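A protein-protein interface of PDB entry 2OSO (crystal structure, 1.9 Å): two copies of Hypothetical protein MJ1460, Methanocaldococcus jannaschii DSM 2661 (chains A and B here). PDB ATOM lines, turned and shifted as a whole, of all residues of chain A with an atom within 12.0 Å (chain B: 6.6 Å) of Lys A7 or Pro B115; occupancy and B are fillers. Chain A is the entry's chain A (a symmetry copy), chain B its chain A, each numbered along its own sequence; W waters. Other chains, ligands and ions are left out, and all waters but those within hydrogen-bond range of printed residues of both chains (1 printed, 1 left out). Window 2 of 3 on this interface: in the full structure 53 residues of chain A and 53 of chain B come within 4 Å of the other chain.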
ATOM      1  N   MET A   2      14.717  20.469  -2.992  1.00  0.00           N
ATOM      2  CA  MET A   2      16.109  20.740  -2.594  1.00  0.00           C
ATOM      3  C   MET A   2      16.474  19.817  -1.448  1.00  0.00           C
ATOM      4  O   MET A   2      15.630  19.566  -0.589  1.00  0.00           O
ATOM      5  CB  MET A   2      16.295  22.203  -2.149  1.00  0.00           C
ATOM      6  CG  MET A   2      16.015  23.286  -3.218  1.00  0.00           C
ATOM      7  SD  MET A   2      17.137  23.169  -4.795  1.00  0.00           S
ATOM      8  CE  MET A   2      16.113  21.954  -5.907  1.00  0.00           C
ATOM      9  N   ALA A   3      17.707  19.300  -1.451  1.00  0.00           N
ATOM     10  CA  ALA A   3      18.181  18.420  -0.387  1.00  0.00           C
ATOM     11  C   ALA A   3      18.163  19.174   0.937  1.00  0.00           C
ATOM     12  O   ALA A   3      17.657  18.652   1.926  1.00  0.00           O
ATOM     13  CB  ALA A   3      19.587  17.906  -0.672  1.00  0.00           C
ATOM     14  N   PHE A   4      18.672  20.410   0.933  1.00  0.00           N
ATOM     15  CA  PHE A   4      18.748  21.252   2.144  1.00  0.00           C
ATOM     16  C   PHE A   4      18.014  22.556   1.936  1.00  0.00           C
ATOM     17  O   PHE A   4      18.292  23.304   0.995  1.00  0.00           O
ATOM     18  CB  PHE A   4      20.205  21.533   2.505  1.00  0.00           C
ATOM     19  CG  PHE A   4      20.962  20.303   2.880  1.00  0.00           C
ATOM     20  CD1 PHE A   4      20.560  19.545   3.971  1.00  0.00           C
ATOM     21  CD2 PHE A   4      22.062  19.888   2.138  1.00  0.00           C
ATOM     22  CE1 PHE A   4      21.241  18.393   4.326  1.00  0.00           C
ATOM     23  CE2 PHE A   4      22.748  18.725   2.477  1.00  0.00           C
ATOM     24  CZ  PHE A   4      22.348  17.991   3.574  1.00  0.00           C
ATOM     25  N   MET A   5      17.047  22.815   2.802  1.00  0.00           N
ATOM     26  CA  MET A   5      16.250  24.019   2.703  1.00  0.00           C
ATOM     27  C   MET A   5      16.919  25.235   3.392  1.00  0.00           C
ATOM     28  O   MET A   5      16.446  26.334   3.216  1.00  0.00           O
ATOM     29  CB  MET A   5      14.836  23.777   3.304  1.00  0.00           C
ATOM     30  CG  MET A   5      14.003  22.655   2.624  1.00  0.00           C
ATOM     31  SD  MET A   5      13.341  23.052   0.790  1.00  0.00           S
ATOM     32  CE  MET A   5      13.166  21.215   0.072  1.00  0.00           C
ATOM     33  N   GLU A   6      17.976  25.040   4.190  1.00  0.00           N
ATOM     34  CA  GLU A   6      18.652  26.137   4.889  1.00  0.00           C
ATOM     35  C   GLU A   6      20.167  26.073   4.715  1.00  0.00           C
ATOM     36  O   GLU A   6      20.727  24.997   4.476  1.00  0.00           O
ATOM     37  CB  GLU A   6      18.332  26.089   6.390  1.00  0.00           C
ATOM     38  CG  GLU A   6      16.867  26.172   6.730  1.00  0.00           C
ATOM     39  CD  GLU A   6      16.276  27.594   6.519  1.00  0.00           C
ATOM     40  OE1 GLU A   6      17.012  28.568   6.292  1.00  0.00           O
ATOM     41  OE2 GLU A   6      15.052  27.722   6.535  1.00  0.00           O
ATOM     42  N   LYS A   7      20.807  27.226   4.899  1.00  0.00           N
ATOM     43  CA  LYS A   7      22.222  27.480   4.528  1.00  0.00           C
ATOM     44  C   LYS A   7      23.233  26.685   5.355  1.00  0.00           C
ATOM     45  O   LYS A   7      24.307  26.255   4.890  1.00  0.00           O
ATOM     46  CB  LYS A   7      22.568  28.978   4.753  1.00  0.00           C
ATOM     47  CG  LYS A   7      21.787  30.004   3.921  1.00  0.00           C
ATOM     48  CD  LYS A   7      21.805  31.403   4.620  1.00  0.00           C
ATOM     49  CE  LYS A   7      21.283  32.505   3.713  1.00  0.00           C
ATOM     50  NZ  LYS A   7      21.043  33.786   4.497  1.00  0.00           N
ATOM     51  N   ILE A   8      22.898  26.544   6.606  1.00  0.00           N
ATOM     52  CA  ILE A   8      23.806  26.037   7.578  1.00  0.00           C
ATOM     53  C   ILE A   8      23.756  24.498   7.566  1.00  0.00           C
ATOM     54  O   ILE A   8      24.674  23.836   8.061  1.00  0.00           O
ATOM     55  CB  ILE A   8      23.452  26.701   8.965  1.00  0.00           C
ATOM     56  CG1 ILE A   8      24.620  26.548   9.926  1.00  0.00           C
ATOM     57  CG2 ILE A   8      22.089  26.198   9.547  1.00  0.00           C
ATOM     58  CD1 ILE A   8      25.684  27.534   9.661  1.00  0.00           C
ATOM     59  N   PHE A   9      22.702  23.909   6.983  1.00  0.00           N
ATOM     60  CA  PHE A   9      22.523  22.433   7.097  1.00  0.00           C
ATOM     61  C   PHE A   9      23.683  21.522   6.575  1.00  0.00           C
ATOM     62  O   PHE A   9      24.092  20.597   7.273  1.00  0.00           O
ATOM     63  CB  PHE A   9      21.173  21.992   6.508  1.00  0.00           C
ATOM     64  CG  PHE A   9      19.981  22.456   7.263  1.00  0.00           C
ATOM     65  CD1 PHE A   9      20.073  22.998   8.549  1.00  0.00           C
ATOM     66  CD2 PHE A   9      18.716  22.245   6.724  1.00  0.00           C
ATOM     67  CE1 PHE A   9      18.908  23.347   9.264  1.00  0.00           C
ATOM     68  CE2 PHE A   9      17.543  22.605   7.448  1.00  0.00           C
ATOM     69  CZ  PHE A   9      17.665  23.163   8.697  1.00  0.00           C
ATOM     70  N   PRO A  10      24.210  21.732   5.355  1.00  0.00           N
ATOM     71  CA  PRO A  10      25.373  20.889   5.056  1.00  0.00           C
ATOM     72  C   PRO A  10      26.544  20.959   6.037  1.00  0.00           C
ATOM     73  O   PRO A  10      27.207  19.966   6.303  1.00  0.00           O
ATOM     74  CB  PRO A  10      25.805  21.337   3.657  1.00  0.00           C
ATOM     75  CG  PRO A  10      25.020  22.625   3.369  1.00  0.00           C
ATOM     76  CD  PRO A  10      23.809  22.588   4.228  1.00  0.00           C
ATOM     77  N   ASP A  11      26.792  22.128   6.572  1.00  0.00           N
ATOM     78  CA  ASP A  11      27.900  22.357   7.496  1.00  0.00           C
ATOM     79  C   ASP A  11      27.651  21.611   8.820  1.00  0.00           C
ATOM     80  O   ASP A  11      28.563  21.009   9.407  1.00  0.00           O
ATOM     81  CB  ASP A  11      28.044  23.882   7.754  1.00  0.00           C
ATOM     82  CG  ASP A  11      28.225  24.681   6.476  1.00  0.00           C
ATOM     83  OD1 ASP A  11      29.308  24.592   5.910  1.00  0.00           O
ATOM     84  OD2 ASP A  11      27.275  25.382   6.039  1.00  0.00           O
ATOM     85  N   ILE A  12      26.411  21.623   9.287  1.00  0.00           N
ATOM     86  CA  ILE A  12      26.064  20.892  10.512  1.00  0.00           C
ATOM     87  C   ILE A  12      26.345  19.386  10.373  1.00  0.00           C
ATOM     88  O   ILE A  12      26.866  18.776  11.304  1.00  0.00           O
ATOM     89  CB  ILE A  12      24.598  21.167  10.975  1.00  0.00           C
ATOM     90  CG1 ILE A  12      24.472  22.586  11.554  1.00  0.00           C
ATOM     91  CG2 ILE A  12      24.156  20.163  12.032  1.00  0.00           C
ATOM     92  CD1 ILE A  12      23.297  23.344  10.981  1.00  0.00           C
ATOM     93  N   LEU A  13      26.057  18.799   9.207  1.00  0.00           N
ATOM     94  CA  LEU A  13      26.324  17.391   8.998  1.00  0.00           C
ATOM     95  C   LEU A  13      27.832  17.062   9.051  1.00  0.00           C
ATOM     96  O   LEU A  13      28.214  15.975   9.466  1.00  0.00           O
ATOM     97  CB  LEU A  13      25.705  16.874   7.691  1.00  0.00           C
ATOM     98  CG  LEU A  13      24.181  16.772   7.561  1.00  0.00           C
ATOM     99  CD1 LEU A  13      23.803  16.224   6.194  1.00  0.00           C
ATOM    100  CD2 LEU A  13      23.615  15.911   8.639  1.00  0.00           C
ATOM    101  N   GLU A  14      28.678  17.999   8.640  1.00  0.00           N
ATOM    102  CA  GLU A  14      30.132  17.809   8.730  1.00  0.00           C
ATOM    103  C   GLU A  14      30.624  17.932  10.176  1.00  0.00           C
ATOM    104  O   GLU A  14      31.433  17.119  10.645  1.00  0.00           O
ATOM    105  CB  GLU A  14      30.844  18.868   7.916  1.00  0.00           C
ATOM    106  CG  GLU A  14      31.137  18.523   6.525  1.00  0.00           C
ATOM    107  CD  GLU A  14      32.105  19.520   5.939  1.00  0.00           C
ATOM    108  OE1 GLU A  14      31.644  20.616   5.530  1.00  0.00           O
ATOM    109  OE2 GLU A  14      33.323  19.230   5.915  1.00  0.00           O
ATOM    110  N   ALA A  15      30.129  18.968  10.852  1.00  0.00           N
ATOM    111  CA  ALA A  15      30.487  19.274  12.246  1.00  0.00           C
ATOM    112  C   ALA A  15      30.163  18.159  13.217  1.00  0.00           C
ATOM    113  O   ALA A  15      30.910  17.960  14.157  1.00  0.00           O
ATOM    114  CB  ALA A  15      29.811  20.569  12.708  1.00  0.00           C
ATOM    115  N   PHE A  36      13.004  26.039  21.163  1.00  0.00           N
ATOM    116  CA  PHE A  36      13.025  25.841  19.719  1.00  0.00           C
ATOM    117  C   PHE A  36      11.995  24.794  19.261  1.00  0.00           C
ATOM    118  O   PHE A  36      11.220  25.013  18.313  1.00  0.00           O
ATOM    119  CB  PHE A  36      14.424  25.461  19.295  1.00  0.00           C
ATOM    120  CG  PHE A  36      14.617  25.454  17.801  1.00  0.00           C
ATOM    121  CD1 PHE A  36      14.900  26.629  17.145  1.00  0.00           C
ATOM    122  CD2 PHE A  36      14.505  24.280  17.076  1.00  0.00           C
ATOM    123  CE1 PHE A  36      15.071  26.661  15.771  1.00  0.00           C
ATOM    124  CE2 PHE A  36      14.660  24.288  15.677  1.00  0.00           C
ATOM    125  CZ  PHE A  36      14.968  25.490  15.036  1.00  0.00           C
ATOM    126  N   LEU B  53      14.068  29.055   8.795  1.00  0.00           N
ATOM    127  CA  LEU B  53      14.735  29.413  10.044  1.00  0.00           C
ATOM    128  C   LEU B  53      14.468  30.887  10.478  1.00  0.00           C
ATOM    129  O   LEU B  53      14.389  31.185  11.666  1.00  0.00           O
ATOM    130  CB  LEU B  53      16.232  29.129   9.936  1.00  0.00           C
ATOM    131  CG  LEU B  53      16.535  27.619  10.114  1.00  0.00           C
ATOM    132  CD1 LEU B  53      17.950  27.341   9.848  1.00  0.00           C
ATOM    133  CD2 LEU B  53      16.190  27.191  11.553  1.00  0.00           C
ATOM    134  N   VAL B 110      32.262  28.058  10.677  1.00  0.00           N
ATOM    135  CA  VAL B 110      31.705  28.058   9.320  1.00  0.00           C
ATOM    136  C   VAL B 110      32.248  29.174   8.422  1.00  0.00           C
ATOM    137  O   VAL B 110      32.253  30.345   8.774  1.00  0.00           O
ATOM    138  CB  VAL B 110      30.149  28.163   9.342  1.00  0.00           C
ATOM    139  CG1 VAL B 110      29.606  28.227   7.943  1.00  0.00           C
ATOM    140  CG2 VAL B 110      29.541  27.008  10.064  1.00  0.00           C
ATOM    141  N   LYS B 112      31.370  30.849   4.674  1.00  0.00           N
ATOM    142  CA  LYS B 112      30.355  30.934   3.625  1.00  0.00           C
ATOM    143  C   LYS B 112      30.403  32.344   2.969  1.00  0.00           C
ATOM    144  O   LYS B 112      30.602  33.338   3.673  1.00  0.00           O
ATOM    145  CB  LYS B 112      28.986  30.661   4.288  1.00  0.00           C
ATOM    146  CG  LYS B 112      27.862  30.334   3.311  1.00  0.00           C
ATOM    147  CD  LYS B 112      26.985  29.154   3.794  1.00  0.00           C
ATOM    148  CE  LYS B 112      27.597  27.841   3.419  1.00  0.00           C
ATOM    149  NZ  LYS B 112      26.813  26.651   3.850  1.00  0.00           N
ATOM    150  N   GLU B 113      30.206  32.436   1.651  1.00  0.00           N
ATOM    151  CA  GLU B 113      30.162  33.738   0.960  1.00  0.00           C
ATOM    152  C   GLU B 113      28.967  34.620   1.312  1.00  0.00           C
ATOM    153  O   GLU B 113      29.022  35.845   1.170  1.00  0.00           O
ATOM    154  CB  GLU B 113      30.173  33.569  -0.570  1.00  0.00           C
ATOM    155  CG  GLU B 113      31.366  32.844  -1.133  1.00  0.00           C
ATOM    156  CD  GLU B 113      31.461  32.985  -2.644  1.00  0.00           C
ATOM    157  OE1 GLU B 113      30.678  33.787  -3.255  1.00  0.00           O
ATOM    158  OE2 GLU B 113      32.340  32.317  -3.230  1.00  0.00           O
ATOM    159  N   GLU B 114      27.882  33.994   1.746  1.00  0.00           N
ATOM    160  CA  GLU B 114      26.656  34.670   2.030  1.00  0.00           C
ATOM    161  C   GLU B 114      26.456  34.619   3.562  1.00  0.00           C
ATOM    162  O   GLU B 114      26.950  33.679   4.225  1.00  0.00           O
ATOM    163  CB  GLU B 114      25.502  33.981   1.300  1.00  0.00           C
ATOM    164  CG  GLU B 114      24.452  34.915   0.761  1.00  0.00           C
ATOM    165  CD  GLU B 114      24.141  34.655  -0.705  1.00  0.00           C
ATOM    166  N   PRO B 115      25.814  35.643   4.117  1.00  0.00           N
ATOM    167  CA  PRO B 115      25.529  35.673   5.572  1.00  0.00           C
ATOM    168  C   PRO B 115      24.727  34.463   6.026  1.00  0.00           C
ATOM    169  O   PRO B 115      23.832  34.020   5.254  1.00  0.00           O
ATOM    170  CB  PRO B 115      24.744  36.996   5.732  1.00  0.00           C
ATOM    171  CG  PRO B 115      25.125  37.812   4.686  1.00  0.00           C
ATOM    172  CD  PRO B 115      25.350  36.897   3.486  1.00  0.00           C
ATOM    173  N   ILE B 116      24.955  33.960   7.266  1.00  0.00           N
ATOM    174  CA  ILE B 116      24.399  32.652   7.677  1.00  0.00           C
ATOM    175  C   ILE B 116      23.369  32.686   8.806  1.00  0.00           C
ATOM    176  O   ILE B 116      22.791  31.694   9.059  1.00  0.00           O
ATOM    177  CB  ILE B 116      25.481  31.559   7.988  1.00  0.00           C
ATOM    178  CG1 ILE B 116      26.422  31.952   9.159  1.00  0.00           C
ATOM    179  CG2 ILE B 116      26.386  31.299   6.670  1.00  0.00           C
ATOM    180  CD1 ILE B 116      27.245  30.831   9.708  1.00  0.00           C
ATOM    181  N   HIS B 117      23.193  33.812   9.470  1.00  0.00           N
ATOM    182  CA  HIS B 117      22.558  33.832  10.771  1.00  0.00           C
ATOM    183  C   HIS B 117      21.087  34.239  10.567  1.00  0.00           C
ATOM    184  O   HIS B 117      20.611  35.199  11.168  1.00  0.00           O
ATOM    185  CB  HIS B 117      23.306  34.740  11.724  1.00  0.00           C
ATOM    186  CG  HIS B 117      24.604  34.179  12.210  1.00  0.00           C
ATOM    187  ND1 HIS B 117      25.833  34.627  11.764  1.00  0.00           N
ATOM    188  CD2 HIS B 117      24.864  33.099  12.978  1.00  0.00           C
ATOM    189  CE1 HIS B 117      26.795  33.928  12.346  1.00  0.00           C
ATOM    190  NE2 HIS B 117      26.230  32.985  13.080  1.00  0.00           N
ATOM    191  N   ASP B 118      20.382  33.443   9.747  1.00  0.00           N
ATOM    192  CA  ASP B 118      18.955  33.651   9.433  1.00  0.00           C
ATOM    193  C   ASP B 118      18.038  33.496  10.668  1.00  0.00           C
ATOM    194  O   ASP B 118      17.079  34.259  10.792  1.00  0.00           O
ATOM    195  CB  ASP B 118      18.429  32.648   8.422  1.00  0.00           C
ATOM    196  CG  ASP B 118      18.929  32.871   7.033  1.00  0.00           C
ATOM    197  OD1 ASP B 118      19.884  33.645   6.826  1.00  0.00           O
ATOM    198  OD2 ASP B 118      18.351  32.209   6.154  1.00  0.00           O
ATOM    199  N   GLU B 140      20.541  40.393   7.290  1.00  0.00           N
ATOM    200  CA  GLU B 140      21.928  40.357   7.687  1.00  0.00           C
ATOM    201  C   GLU B 140      22.691  40.679   6.415  1.00  0.00           C
ATOM    202  O   GLU B 140      22.518  40.002   5.406  1.00  0.00           O
ATOM    203  CB  GLU B 140      22.346  38.980   8.280  1.00  0.00           C
ATOM    204  CG  GLU B 140      23.781  38.981   8.829  1.00  0.00           C
ATOM    205  CD  GLU B 140      24.201  37.648   9.411  1.00  0.00           C
ATOM    206  OE1 GLU B 140      23.578  36.629   9.066  1.00  0.00           O
ATOM    207  OE2 GLU B 140      25.177  37.610  10.195  1.00  0.00           O
ATOM    208  N   VAL B 141      23.519  41.718   6.482  1.00  0.00           N
ATOM    209  CA  VAL B 141      24.240  42.224   5.319  1.00  0.00           C
ATOM    210  C   VAL B 141      25.736  41.985   5.432  1.00  0.00           C
ATOM    211  O   VAL B 141      26.432  42.056   4.432  1.00  0.00           O
ATOM    212  CB  VAL B 141      23.915  43.752   5.116  1.00  0.00           C
ATOM    213  CG1 VAL B 141      22.361  43.998   4.901  1.00  0.00           C
ATOM    214  CG2 VAL B 141      24.429  44.589   6.329  1.00  0.00           C
ATOM    215  N   GLU B 142      26.262  41.759   6.634  1.00  0.00           N
ATOM    216  CA  GLU B 142      27.668  41.296   6.780  1.00  0.00           C
ATOM    217  C   GLU B 142      27.716  40.213   7.860  1.00  0.00           C
ATOM    218  O   GLU B 142      26.917  40.235   8.801  1.00  0.00           O
ATOM    219  CB  GLU B 142      28.645  42.423   7.181  1.00  0.00           C
ATOM    220  CG  GLU B 142      28.558  43.710   6.430  1.00  0.00           C
ATOM    221  CD  GLU B 142      29.552  44.781   6.951  1.00  0.00           C
ATOM    222  OE1 GLU B 142      30.461  44.479   7.756  1.00  0.00           O
ATOM    223  OE2 GLU B 142      29.401  45.946   6.561  1.00  0.00           O
ATOM    224  N   CYS B 143      28.679  39.305   7.777  1.00  0.00           N
ATOM    225  CA  CYS B 143      28.670  38.133   8.707  1.00  0.00           C
ATOM    226  C   CYS B 143      30.114  37.666   8.992  1.00  0.00           C
ATOM    227  O   CYS B 143      30.970  37.747   8.126  1.00  0.00           O
ATOM    228  CB  CYS B 143      27.821  37.036   8.074  1.00  0.00           C
ATOM    229  SG  CYS B 143      27.625  35.497   8.979  1.00  0.00           S
ATOM    230  N   SER B 145      31.114  34.782   9.273  1.00  0.00           N
ATOM    231  CA  SER B 145      31.446  33.629   8.443  1.00  0.00           C
ATOM    232  C   SER B 145      31.885  34.036   7.036  1.00  0.00           C
ATOM    233  O   SER B 145      32.397  33.204   6.280  1.00  0.00           O
ATOM    234  CB  SER B 145      30.288  32.625   8.456  1.00  0.00           C
ATOM    235  OG  SER B 145      30.154  32.033   9.753  1.00  0.00           O
ATOM    236  N   GLN B 146      31.731  35.321   6.700  1.00  0.00           N
ATOM    237  CA  GLN B 146      32.377  35.899   5.502  1.00  0.00           C
ATOM    238  C   GLN B 146      33.810  36.390   5.750  1.00  0.00           C
ATOM    239  O   GLN B 146      34.443  36.883   4.837  1.00  0.00           O
ATOM    240  CB  GLN B 146      31.596  37.087   4.938  1.00  0.00           C
ATOM    241  CG  GLN B 146      30.103  36.826   4.630  1.00  0.00           C
ATOM    242  CD  GLN B 146      29.393  38.135   4.261  1.00  0.00           C
ATOM    243  OE1 GLN B 146      29.489  39.112   4.990  1.00  0.00           O
ATOM    244  NE2 GLN B 146      28.710  38.160   3.112  1.00  0.00           N
ATOM    245  N   VAL B 152      26.506  42.108  10.915  1.00  0.00           N
ATOM    246  CA  VAL B 152      25.763  43.350  10.802  1.00  0.00           C
ATOM    247  C   VAL B 152      24.386  43.096  10.198  1.00  0.00           C
ATOM    248  O   VAL B 152      24.242  42.491   9.134  1.00  0.00           O
ATOM    249  CB  VAL B 152      26.506  44.389   9.974  1.00  0.00           C
ATOM    250  CG1 VAL B 152      25.675  45.684   9.874  1.00  0.00           C
ATOM    251  CG2 VAL B 152      27.895  44.662  10.544  1.00  0.00           C
HETATM  252  O   HOH W   1      15.867  31.110   6.852  1.00  0.00           O
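Printed residues of chain A that touch a printed residue of chain B: Glu A6, Lys A7, Ile A8 and Asp A11. Hydrophobic or aromatic side chains of chain A that line the printed part of chain B: Ile A8. Hydrophobic or aromatic side chains of chain B that line the printed part of chain A: Leu B53, Val B110 and Ile B116.
No position is printed for both chains. Of the 8 pairs that touch across the chains among the printed residues, none has its exchanged pair printed and touching as well.
O of Val B110 is in hydrogen-bond range of OG of Ser B145. The backbone carbonyl oxygen of Ser B145 is in hydrogen-bond range of the backbone NH of Lys B112, 3.0 Å away. N of Ile B116 sits close to SG of Cys B143 (3.5 Å).
Water W1 lies within hydrogen-bond range of the side-chain carboxylate of Asp B118 (2.8 Å), the side-chain carboxylate of Glu A6 (2.8 Å) and the backbone NH of Leu B53 (3.4 Å).
Among the printed residues, pairs that only touch across the chains: Glu A6 with Asp B118, Ile A8 with Val B110 and Ile A8 with Ile B116.
The side-chain carboxylate of Glu A6 is in hydrogen-bond range of the backbone NH of Leu B53, 2.8 Å away. O of Lys A7 sits at hydrogen-bond distance from NZ of Lys B112 (2.7 Å). The side-chain amino group (NZ) of Lys B112 is in salt-bridge range of the side-chain carboxylate (OD2) of Asp A11, at 2.6 Å. NZ of Lys A7 lies within hydrogen-bond range of O of Pro B115 (2.9 Å). The side-chain amino group (NZ) of Lys A7 is in salt-bridge range of the side-chain carboxylate (OD1) of Asp B118 (2.6 Å).
Of chain B, only Lys B112 (2.7 Å), Pro B115 (2.9 Å) and Asp B118 (2.6 Å) come within 4 Å of Lys A7. Pro B115 touches just one residue of chain A: Lys A7 (2.9 Å). Of chain A, only Lys A7 and Asp A11 come within 4 Å of Lys B112. No residue of chain A comes within 4 Å of Glu B114. Of chain A, only Ile A8 comes within 4 Å of Ile B116. No residue of chain A comes within 4 Å of His B117. Of the printed residues of chain A, Asp B118 touches Glu A6 (3.9 Å) and Lys A7 (2.6 Å). No residue of chain A comes within 4 Å of Glu B140. No residue of chain A comes within 4 Å of Val B141. No residue of chain A comes within 4 Å of Cys B143. Of the printed residues of chain B, Ile A8 touches Val B110 and Ile B116. Of the printed residues of chain B, Glu A6 touches Leu B53 (2.8 Å) and Asp B118 (3.9 Å). Printed residues of chain A within 4 Å of Val B110: Ile A8. Of the printed residues of chain B, Asp A11 touches Lys B112 (2.6 Å). Printed residues of chain A within 4 Å of Leu B53: Glu A6. Glu B113 touches none of the printed residues of chain A. Phe A4 touches none of the printed residues of chain B. The nearest residue of chain B that does not touch Lys A7 is Ile B116 (4.2 Å).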
